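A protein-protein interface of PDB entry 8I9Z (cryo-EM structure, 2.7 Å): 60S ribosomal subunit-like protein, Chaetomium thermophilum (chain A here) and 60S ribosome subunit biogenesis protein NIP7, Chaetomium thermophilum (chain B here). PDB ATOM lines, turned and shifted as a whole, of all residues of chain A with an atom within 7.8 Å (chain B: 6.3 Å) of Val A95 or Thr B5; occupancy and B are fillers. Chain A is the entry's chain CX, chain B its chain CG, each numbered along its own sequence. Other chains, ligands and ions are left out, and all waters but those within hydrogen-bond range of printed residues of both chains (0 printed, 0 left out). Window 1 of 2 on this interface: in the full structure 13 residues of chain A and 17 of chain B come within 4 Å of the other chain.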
ATOM      1  N   LYS A  90       0.540  29.666 -26.982  1.00  0.00           N
ATOM      2  CA  LYS A  90       0.582  28.411 -27.730  1.00  0.00           C
ATOM      3  C   LYS A  90       0.072  27.295 -26.821  1.00  0.00           C
ATOM      4  O   LYS A  90       0.818  26.692 -26.047  1.00  0.00           O
ATOM      5  CB  LYS A  90       1.993  28.126 -28.225  1.00  0.00           C
ATOM      6  CG  LYS A  90       2.473  29.056 -29.321  1.00  0.00           C
ATOM      7  CD  LYS A  90       3.620  28.448 -30.121  1.00  0.00           C
ATOM      8  CE  LYS A  90       4.800  28.038 -29.251  1.00  0.00           C
ATOM      9  NZ  LYS A  90       5.147  29.049 -28.215  1.00  0.00           N
ATOM     10  N   GLY A  91      -1.232  27.038 -26.931  1.00  0.00           N
ATOM     11  CA  GLY A  91      -1.936  26.143 -26.032  1.00  0.00           C
ATOM     12  C   GLY A  91      -1.374  24.740 -25.935  1.00  0.00           C
ATOM     13  O   GLY A  91      -1.231  24.043 -26.942  1.00  0.00           O
ATOM     14  N   LYS A  92      -1.041  24.328 -24.717  1.00  0.00           N
ATOM     15  CA  LYS A  92      -0.357  23.064 -24.491  1.00  0.00           C
ATOM     16  C   LYS A  92      -1.314  21.896 -24.664  1.00  0.00           C
ATOM     17  O   LYS A  92      -2.398  21.876 -24.073  1.00  0.00           O
ATOM     18  CB  LYS A  92       0.249  23.032 -23.089  1.00  0.00           C
ATOM     19  CG  LYS A  92       1.093  24.238 -22.731  1.00  0.00           C
ATOM     20  CD  LYS A  92       1.041  24.504 -21.235  1.00  0.00           C
ATOM     21  CE  LYS A  92       2.404  24.385 -20.591  1.00  0.00           C
ATOM     22  NZ  LYS A  92       3.201  25.632 -20.733  1.00  0.00           N
ATOM     23  N   VAL A  93      -0.910  20.919 -25.467  1.00  0.00           N
ATOM     24  CA  VAL A  93      -1.616  19.652 -25.599  1.00  0.00           C
ATOM     25  C   VAL A  93      -0.773  18.574 -24.926  1.00  0.00           C
ATOM     26  O   VAL A  93       0.456  18.563 -25.060  1.00  0.00           O
ATOM     27  CB  VAL A  93      -1.930  19.323 -27.071  1.00  0.00           C
ATOM     28  CG1 VAL A  93      -2.862  20.372 -27.644  1.00  0.00           C
ATOM     29  CG2 VAL A  93      -0.669  19.271 -27.919  1.00  0.00           C
ATOM     30  N   PHE A  94      -1.422  17.711 -24.152  1.00  0.00           N
ATOM     31  CA  PHE A  94      -0.718  16.755 -23.312  1.00  0.00           C
ATOM     32  C   PHE A  94      -0.756  15.359 -23.917  1.00  0.00           C
ATOM     33  O   PHE A  94      -1.702  14.985 -24.613  1.00  0.00           O
ATOM     34  CB  PHE A  94      -1.305  16.726 -21.902  1.00  0.00           C
ATOM     35  CG  PHE A  94      -1.018  17.961 -21.106  1.00  0.00           C
ATOM     36  CD1 PHE A  94       0.206  18.591 -21.200  1.00  0.00           C
ATOM     37  CD2 PHE A  94      -1.975  18.492 -20.264  1.00  0.00           C
ATOM     38  CE1 PHE A  94       0.470  19.726 -20.475  1.00  0.00           C
ATOM     39  CE2 PHE A  94      -1.713  19.628 -19.536  1.00  0.00           C
ATOM     40  CZ  PHE A  94      -0.489  20.244 -19.642  1.00  0.00           C
ATOM     41  N   VAL A  95       0.290  14.590 -23.631  1.00  0.00           N
ATOM     42  CA  VAL A  95       0.509  13.279 -24.228  1.00  0.00           C
ATOM     43  C   VAL A  95       0.546  12.258 -23.089  1.00  0.00           C
ATOM     44  O   VAL A  95       1.253  11.242 -23.140  1.00  0.00           O
ATOM     45  CB  VAL A  95       1.779  13.315 -25.112  1.00  0.00           C
ATOM     46  CG1 VAL A  95       3.047  13.560 -24.294  1.00  0.00           C
ATOM     47  CG2 VAL A  95       1.889  12.114 -26.069  1.00  0.00           C
ATOM     48  N   ASP A  96      -0.252  12.520 -22.051  1.00  0.00           N
ATOM     49  CA  ASP A  96      -0.309  11.637 -20.888  1.00  0.00           C
ATOM     50  C   ASP A  96      -0.875  10.263 -21.228  1.00  0.00           C
ATOM     51  O   ASP A  96      -0.612   9.293 -20.509  1.00  0.00           O
ATOM     52  CB  ASP A  96      -1.151  12.289 -19.790  1.00  0.00           C
ATOM     53  CG  ASP A  96      -0.962  11.633 -18.438  1.00  0.00           C
ATOM     54  OD1 ASP A  96       0.041  10.913 -18.253  1.00  0.00           O
ATOM     55  OD2 ASP A  96      -1.823  11.834 -17.556  1.00  0.00           O
ATOM     56  N   ASP A  97      -1.654  10.157 -22.303  1.00  0.00           N
ATOM     57  CA  ASP A  97      -2.241   8.881 -22.687  1.00  0.00           C
ATOM     58  C   ASP A  97      -1.165   7.901 -23.132  1.00  0.00           C
ATOM     59  O   ASP A  97      -0.209   8.272 -23.819  1.00  0.00           O
ATOM     60  CB  ASP A  97      -3.261   9.087 -23.808  1.00  0.00           C
ATOM     61  CG  ASP A  97      -4.528   9.770 -23.329  1.00  0.00           C
ATOM     62  OD1 ASP A  97      -4.710   9.894 -22.100  1.00  0.00           O
ATOM     63  OD2 ASP A  97      -5.342  10.183 -24.182  1.00  0.00           O
ATOM     64  N   ARG A  98      -1.321   6.642 -22.720  1.00  0.00           N
ATOM     65  CA  ARG A  98      -0.338   5.613 -23.047  1.00  0.00           C
ATOM     66  C   ARG A  98      -0.309   5.305 -24.540  1.00  0.00           C
ATOM     67  O   ARG A  98       0.767   5.066 -25.102  1.00  0.00           O
ATOM     68  CB  ARG A  98      -0.628   4.357 -22.228  1.00  0.00           C
ATOM     69  CG  ARG A  98      -0.263   3.057 -22.899  1.00  0.00           C
ATOM     70  CD  ARG A  98       0.170   2.028 -21.892  1.00  0.00           C
ATOM     71  NE  ARG A  98       0.149   0.688 -22.460  1.00  0.00           N
ATOM     72  CZ  ARG A  98      -0.919  -0.096 -22.483  1.00  0.00           C
ATOM     73  NH1 ARG A  98      -2.074   0.296 -21.969  1.00  0.00           N
ATOM     74  NH2 ARG A  98      -0.825  -1.303 -23.030  1.00  0.00           N
ATOM     75  N   GLU A  99      -1.469   5.318 -25.198  1.00  0.00           N
ATOM     76  CA  GLU A  99      -1.511   5.125 -26.642  1.00  0.00           C
ATOM     77  C   GLU A  99      -0.821   6.268 -27.374  1.00  0.00           C
ATOM     78  O   GLU A  99      -0.124   6.042 -28.368  1.00  0.00           O
ATOM     79  CB  GLU A  99      -2.959   4.983 -27.107  1.00  0.00           C
ATOM     80  CG  GLU A  99      -3.600   3.622 -26.829  1.00  0.00           C
ATOM     81  CD  GLU A  99      -4.032   3.405 -25.380  1.00  0.00           C
ATOM     82  OE1 GLU A  99      -3.640   4.182 -24.485  1.00  0.00           O
ATOM     83  OE2 GLU A  99      -4.775   2.433 -25.135  1.00  0.00           O
ATOM     84  N   SER A 100      -1.006   7.500 -26.899  1.00  0.00           N
ATOM     85  CA  SER A 100      -0.275   8.628 -27.466  1.00  0.00           C
ATOM     86  C   SER A 100       1.199   8.563 -27.095  1.00  0.00           C
ATOM     87  O   SER A 100       2.048   9.146 -27.775  1.00  0.00           O
ATOM     88  CB  SER A 100      -0.897   9.941 -26.996  1.00  0.00           C
ATOM     89  OG  SER A 100      -2.309   9.874 -27.027  1.00  0.00           O
ATOM     90  N   MET A 101       1.517   7.865 -26.008  1.00  0.00           N
ATOM     91  CA  MET A 101       2.907   7.655 -25.625  1.00  0.00           C
ATOM     92  C   MET A 101       3.558   6.572 -26.477  1.00  0.00           C
ATOM     93  O   MET A 101       4.767   6.608 -26.722  1.00  0.00           O
ATOM     94  CB  MET A 101       2.960   7.308 -24.138  1.00  0.00           C
ATOM     95  CG  MET A 101       3.168   8.514 -23.246  1.00  0.00           C
ATOM     96  SD  MET A 101       4.017   8.158 -21.698  1.00  0.00           S
ATOM     97  CE  MET A 101       2.744   7.273 -20.807  1.00  0.00           C
ATOM     98  N   ASN A 102       2.767   5.605 -26.948  1.00  0.00           N
ATOM     99  CA  ASN A 102       3.321   4.516 -27.747  1.00  0.00           C
ATOM    100  C   ASN A 102       3.671   4.970 -29.158  1.00  0.00           C
ATOM    101  O   ASN A 102       4.679   4.531 -29.721  1.00  0.00           O
ATOM    102  CB  ASN A 102       2.346   3.342 -27.799  1.00  0.00           C
ATOM    103  CG  ASN A 102       2.575   2.350 -26.691  1.00  0.00           C
ATOM    104  OD1 ASN A 102       3.714   2.004 -26.385  1.00  0.00           O
ATOM    105  ND2 ASN A 102       1.496   1.871 -26.087  1.00  0.00           N
ATOM    106  N   THR A 103       2.841   5.828 -29.754  1.00  0.00           N
ATOM    107  CA  THR A 103       3.096   6.251 -31.127  1.00  0.00           C
ATOM    108  C   THR A 103       4.329   7.142 -31.221  1.00  0.00           C
ATOM    109  O   THR A 103       5.093   7.039 -32.184  1.00  0.00           O
ATOM    110  CB  THR A 103       1.868   6.951 -31.713  1.00  0.00           C
ATOM    111  OG1 THR A 103       2.243   7.663 -32.897  1.00  0.00           O
ATOM    112  CG2 THR A 103       1.269   7.915 -30.728  1.00  0.00           C
ATOM    113  N   ILE A 104       4.551   8.005 -30.226  1.00  0.00           N
ATOM    114  CA  ILE A 104       5.779   8.796 -30.183  1.00  0.00           C
ATOM    115  C   ILE A 104       6.984   7.885 -29.998  1.00  0.00           C
ATOM    116  O   ILE A 104       8.019   8.060 -30.648  1.00  0.00           O
ATOM    117  CB  ILE A 104       5.691   9.865 -29.076  1.00  0.00           C
ATOM    118  CG1 ILE A 104       4.739  10.986 -29.497  1.00  0.00           C
ATOM    119  CG2 ILE A 104       7.059  10.436 -28.744  1.00  0.00           C
ATOM    120  CD1 ILE A 104       4.832  12.244 -28.650  1.00  0.00           C
ATOM    121  N   GLU A 136      -4.178   4.922 -31.571  1.00  0.00           N
ATOM    122  CA  GLU A 136      -4.306   6.236 -30.951  1.00  0.00           C
ATOM    123  C   GLU A 136      -5.462   7.022 -31.553  1.00  0.00           C
ATOM    124  O   GLU A 136      -6.157   7.760 -30.845  1.00  0.00           O
ATOM    125  CB  GLU A 136      -2.999   7.009 -31.099  1.00  0.00           C
ATOM    126  CG  GLU A 136      -2.951   8.312 -30.339  1.00  0.00           C
ATOM    127  CD  GLU A 136      -2.087   9.347 -31.026  1.00  0.00           C
ATOM    128  OE1 GLU A 136      -1.544   9.045 -32.108  1.00  0.00           O
ATOM    129  OE2 GLU A 136      -1.950  10.464 -30.485  1.00  0.00           O
ATOM    130  N   LYS A 140      -8.771   8.516 -29.652  1.00  0.00           N
ATOM    131  CA  LYS A 140      -9.093   9.937 -29.711  1.00  0.00           C
ATOM    132  C   LYS A 140     -10.495  10.167 -30.259  1.00  0.00           C
ATOM    133  O   LYS A 140     -11.177  11.114 -29.851  1.00  0.00           O
ATOM    134  CB  LYS A 140      -8.054  10.672 -30.556  1.00  0.00           C
ATOM    135  CG  LYS A 140      -6.728  10.905 -29.847  1.00  0.00           C
ATOM    136  CD  LYS A 140      -6.004  12.109 -30.425  1.00  0.00           C
ATOM    137  CE  LYS A 140      -4.781  12.470 -29.600  1.00  0.00           C
ATOM    138  NZ  LYS A 140      -4.195  13.772 -30.025  1.00  0.00           N
ATOM    139  N   ARG B   2       2.586  19.405 -14.271  1.00  0.00           N
ATOM    140  CA  ARG B   2       1.858  19.096 -15.489  1.00  0.00           C
ATOM    141  C   ARG B   2       2.560  17.947 -16.195  1.00  0.00           C
ATOM    142  O   ARG B   2       3.757  17.725 -15.991  1.00  0.00           O
ATOM    143  CB  ARG B   2       1.781  20.314 -16.417  1.00  0.00           C
ATOM    144  CG  ARG B   2       3.121  20.764 -16.930  1.00  0.00           C
ATOM    145  CD  ARG B   2       2.975  21.734 -18.064  1.00  0.00           C
ATOM    146  NE  ARG B   2       4.264  22.256 -18.492  1.00  0.00           N
ATOM    147  CZ  ARG B   2       5.078  21.649 -19.343  1.00  0.00           C
ATOM    148  NH1 ARG B   2       4.765  20.486 -19.888  1.00  0.00           N
ATOM    149  NH2 ARG B   2       6.231  22.225 -19.658  1.00  0.00           N
ATOM    150  N   PRO B   3       1.837  17.184 -17.008  1.00  0.00           N
ATOM    151  CA  PRO B   3       2.496  16.188 -17.854  1.00  0.00           C
ATOM    152  C   PRO B   3       3.194  16.851 -19.031  1.00  0.00           C
ATOM    153  O   PRO B   3       2.994  18.027 -19.332  1.00  0.00           O
ATOM    154  CB  PRO B   3       1.346  15.292 -18.313  1.00  0.00           C
ATOM    155  CG  PRO B   3       0.144  16.132 -18.187  1.00  0.00           C
ATOM    156  CD  PRO B   3       0.374  17.039 -17.030  1.00  0.00           C
ATOM    157  N   LEU B   4       4.033  16.069 -19.703  1.00  0.00           N
ATOM    158  CA  LEU B   4       4.786  16.585 -20.832  1.00  0.00           C
ATOM    159  C   LEU B   4       3.880  16.774 -22.047  1.00  0.00           C
ATOM    160  O   LEU B   4       2.805  16.183 -22.155  1.00  0.00           O
ATOM    161  CB  LEU B   4       5.938  15.648 -21.185  1.00  0.00           C
ATOM    162  CG  LEU B   4       6.877  15.240 -20.051  1.00  0.00           C
ATOM    163  CD1 LEU B   4       7.954  14.312 -20.561  1.00  0.00           C
ATOM    164  CD2 LEU B   4       7.491  16.446 -19.400  1.00  0.00           C
ATOM    165  N   THR B   5       4.330  17.619 -22.968  1.00  0.00           N
ATOM    166  CA  THR B   5       3.635  17.821 -24.225  1.00  0.00           C
ATOM    167  C   THR B   5       4.237  16.915 -25.297  1.00  0.00           C
ATOM    168  O   THR B   5       5.069  16.050 -25.017  1.00  0.00           O
ATOM    169  CB  THR B   5       3.703  19.288 -24.643  1.00  0.00           C
ATOM    170  OG1 THR B   5       5.048  19.625 -24.986  1.00  0.00           O
ATOM    171  CG2 THR B   5       3.242  20.184 -23.510  1.00  0.00           C
ATOM    172  N   ASP B   6       3.809  17.113 -26.544  1.00  0.00           N
ATOM    173  CA  ASP B   6       4.304  16.288 -27.642  1.00  0.00           C
ATOM    174  C   ASP B   6       5.771  16.577 -27.931  1.00  0.00           C
ATOM    175  O   ASP B   6       6.557  15.661 -28.190  1.00  0.00           O
ATOM    176  CB  ASP B   6       3.459  16.520 -28.893  1.00  0.00           C
ATOM    177  CG  ASP B   6       2.004  16.149 -28.691  1.00  0.00           C
ATOM    178  OD1 ASP B   6       1.728  15.251 -27.869  1.00  0.00           O
ATOM    179  OD2 ASP B   6       1.139  16.755 -29.356  1.00  0.00           O
ATOM    180  N   GLN B   7       6.153  17.854 -27.908  1.00  0.00           N
ATOM    181  CA  GLN B   7       7.539  18.210 -28.173  1.00  0.00           C
ATOM    182  C   GLN B   7       8.447  17.786 -27.028  1.00  0.00           C
ATOM    183  O   GLN B   7       9.573  17.338 -27.258  1.00  0.00           O
ATOM    184  CB  GLN B   7       7.662  19.712 -28.423  1.00  0.00           C
ATOM    185  CG  GLN B   7       6.942  20.198 -29.666  1.00  0.00           C
ATOM    186  CD  GLN B   7       7.728  21.261 -30.413  1.00  0.00           C
ATOM    187  OE1 GLN B   7       8.390  22.102 -29.805  1.00  0.00           O
ATOM    188  NE2 GLN B   7       7.660  21.225 -31.738  1.00  0.00           N
ATOM    189  N   GLU B   8       7.973  17.918 -25.790  1.00  0.00           N
ATOM    190  CA  GLU B   8       8.819  17.610 -24.643  1.00  0.00           C
ATOM    191  C   GLU B   8       9.065  16.113 -24.518  1.00  0.00           C
ATOM    192  O   GLU B   8      10.159  15.686 -24.134  1.00  0.00           O
ATOM    193  CB  GLU B   8       8.189  18.159 -23.364  1.00  0.00           C
ATOM    194  CG  GLU B   8       7.869  19.643 -23.411  1.00  0.00           C
ATOM    195  CD  GLU B   8       7.139  20.121 -22.174  1.00  0.00           C
ATOM    196  OE1 GLU B   8       6.577  19.275 -21.453  1.00  0.00           O
ATOM    197  OE2 GLU B   8       7.133  21.343 -21.922  1.00  0.00           O
ATOM    198  N   MET B   9       8.065  15.302 -24.850  1.00  0.00           N
ATOM    199  CA  MET B   9       8.197  13.858 -24.692  1.00  0.00           C
ATOM    200  C   MET B   9       9.043  13.254 -25.807  1.00  0.00           C
ATOM    201  O   MET B   9       9.707  12.232 -25.606  1.00  0.00           O
ATOM    202  CB  MET B   9       6.802  13.240 -24.619  1.00  0.00           C
ATOM    203  CG  MET B   9       6.721  11.742 -24.678  1.00  0.00           C
ATOM    204  SD  MET B   9       6.908  11.093 -23.019  1.00  0.00           S
ATOM    205  CE  MET B   9       5.289  11.422 -22.356  1.00  0.00           C
ATOM    206  N   LYS B  10       9.053  13.888 -26.978  1.00  0.00           N
ATOM    207  CA  LYS B  10       9.970  13.478 -28.036  1.00  0.00           C
ATOM    208  C   LYS B  10      11.420  13.698 -27.621  1.00  0.00           C
ATOM    209  O   LYS B  10      12.291  12.868 -27.898  1.00  0.00           O
ATOM    210  CB  LYS B  10       9.657  14.241 -29.321  1.00  0.00           C
ATOM    211  CG  LYS B  10      10.422  13.755 -30.532  1.00  0.00           C
ATOM    212  CD  LYS B  10       9.610  13.917 -31.801  1.00  0.00           C
ATOM    213  CE  LYS B  10      10.484  14.360 -32.964  1.00  0.00           C
ATOM    214  NZ  LYS B  10      11.114  13.215 -33.681  1.00  0.00           N
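The backbone NH of Val A95 is in hydrogen-bond range of the backbone carbonyl oxygen of Leu B4 (3.3 Å).
Lys A92 touches Arg B2. Val A93 touches Thr B5. CZ of Phe A94 touches CB of Arg B2, at 3.9 Å. Phe A94 touches Pro B3 (CE1 to O, 3.3 Å). Leu B4 touches Phe A94 (O to CD1, 3.7 Å). Val A95 touches Thr B5. Val A95 touches Asp B6 (CB to OD1, 3.4 Å). Val A95 touches Met B9 (CG1 to CE, 3.7 Å). Met A101 touches Met B9. CD1 of Ile A104 touches O of Asp B6, at 3.9 Å.
Printed residues of chain B that touch a printed residue of chain A: Arg B2, Pro B3, Leu B4, Thr B5, Asp B6 and Met B9. Hydrophobic or aromatic side chains of chain B within 4 Å of the printed part of chain A: Pro B3 and Met B9. Along chain B the printed residues that touch a printed residue of chain A span positions 2 to 9. Printed residues of chain A that touch a printed residue of chain B: Lys A92, Val A93, Phe A94, Val A95, Met A101 and Ile A104. Hydrophobic or aromatic side chains of chain A that line the printed part of chain B: Val A93, Phe A94, Val A95, Met A101 and Ile A104. Among the printed residues, no Asp or Glu carboxylate lies within 4 Å of a Lys or Arg side-chain nitrogen of the other chain.
NH2 of Arg B2 lies within salt-bridge range of OE2 of Glu B8, 2.6 Å away. N of Thr B5 lies within hydrogen-bond range of OE1 of Glu B8, 3.2 Å away.
Of the printed residues of chain B, Lys A92 touches Arg B2 (3.5 Å). Printed residues of chain B within 4 Å of Val A93: Thr B5 (3.4 Å) and Asp B6 (3.4 Å). Of chain A, only Val A93 and Val A95 come within 4 Å of Thr B5. Of the printed residues of chain A, Asp B6 touches Val A93, Val A95 and Ile A104. The nearest printed residue of chain A that does not touch Thr B5 is Phe A94 (4.1 Å).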
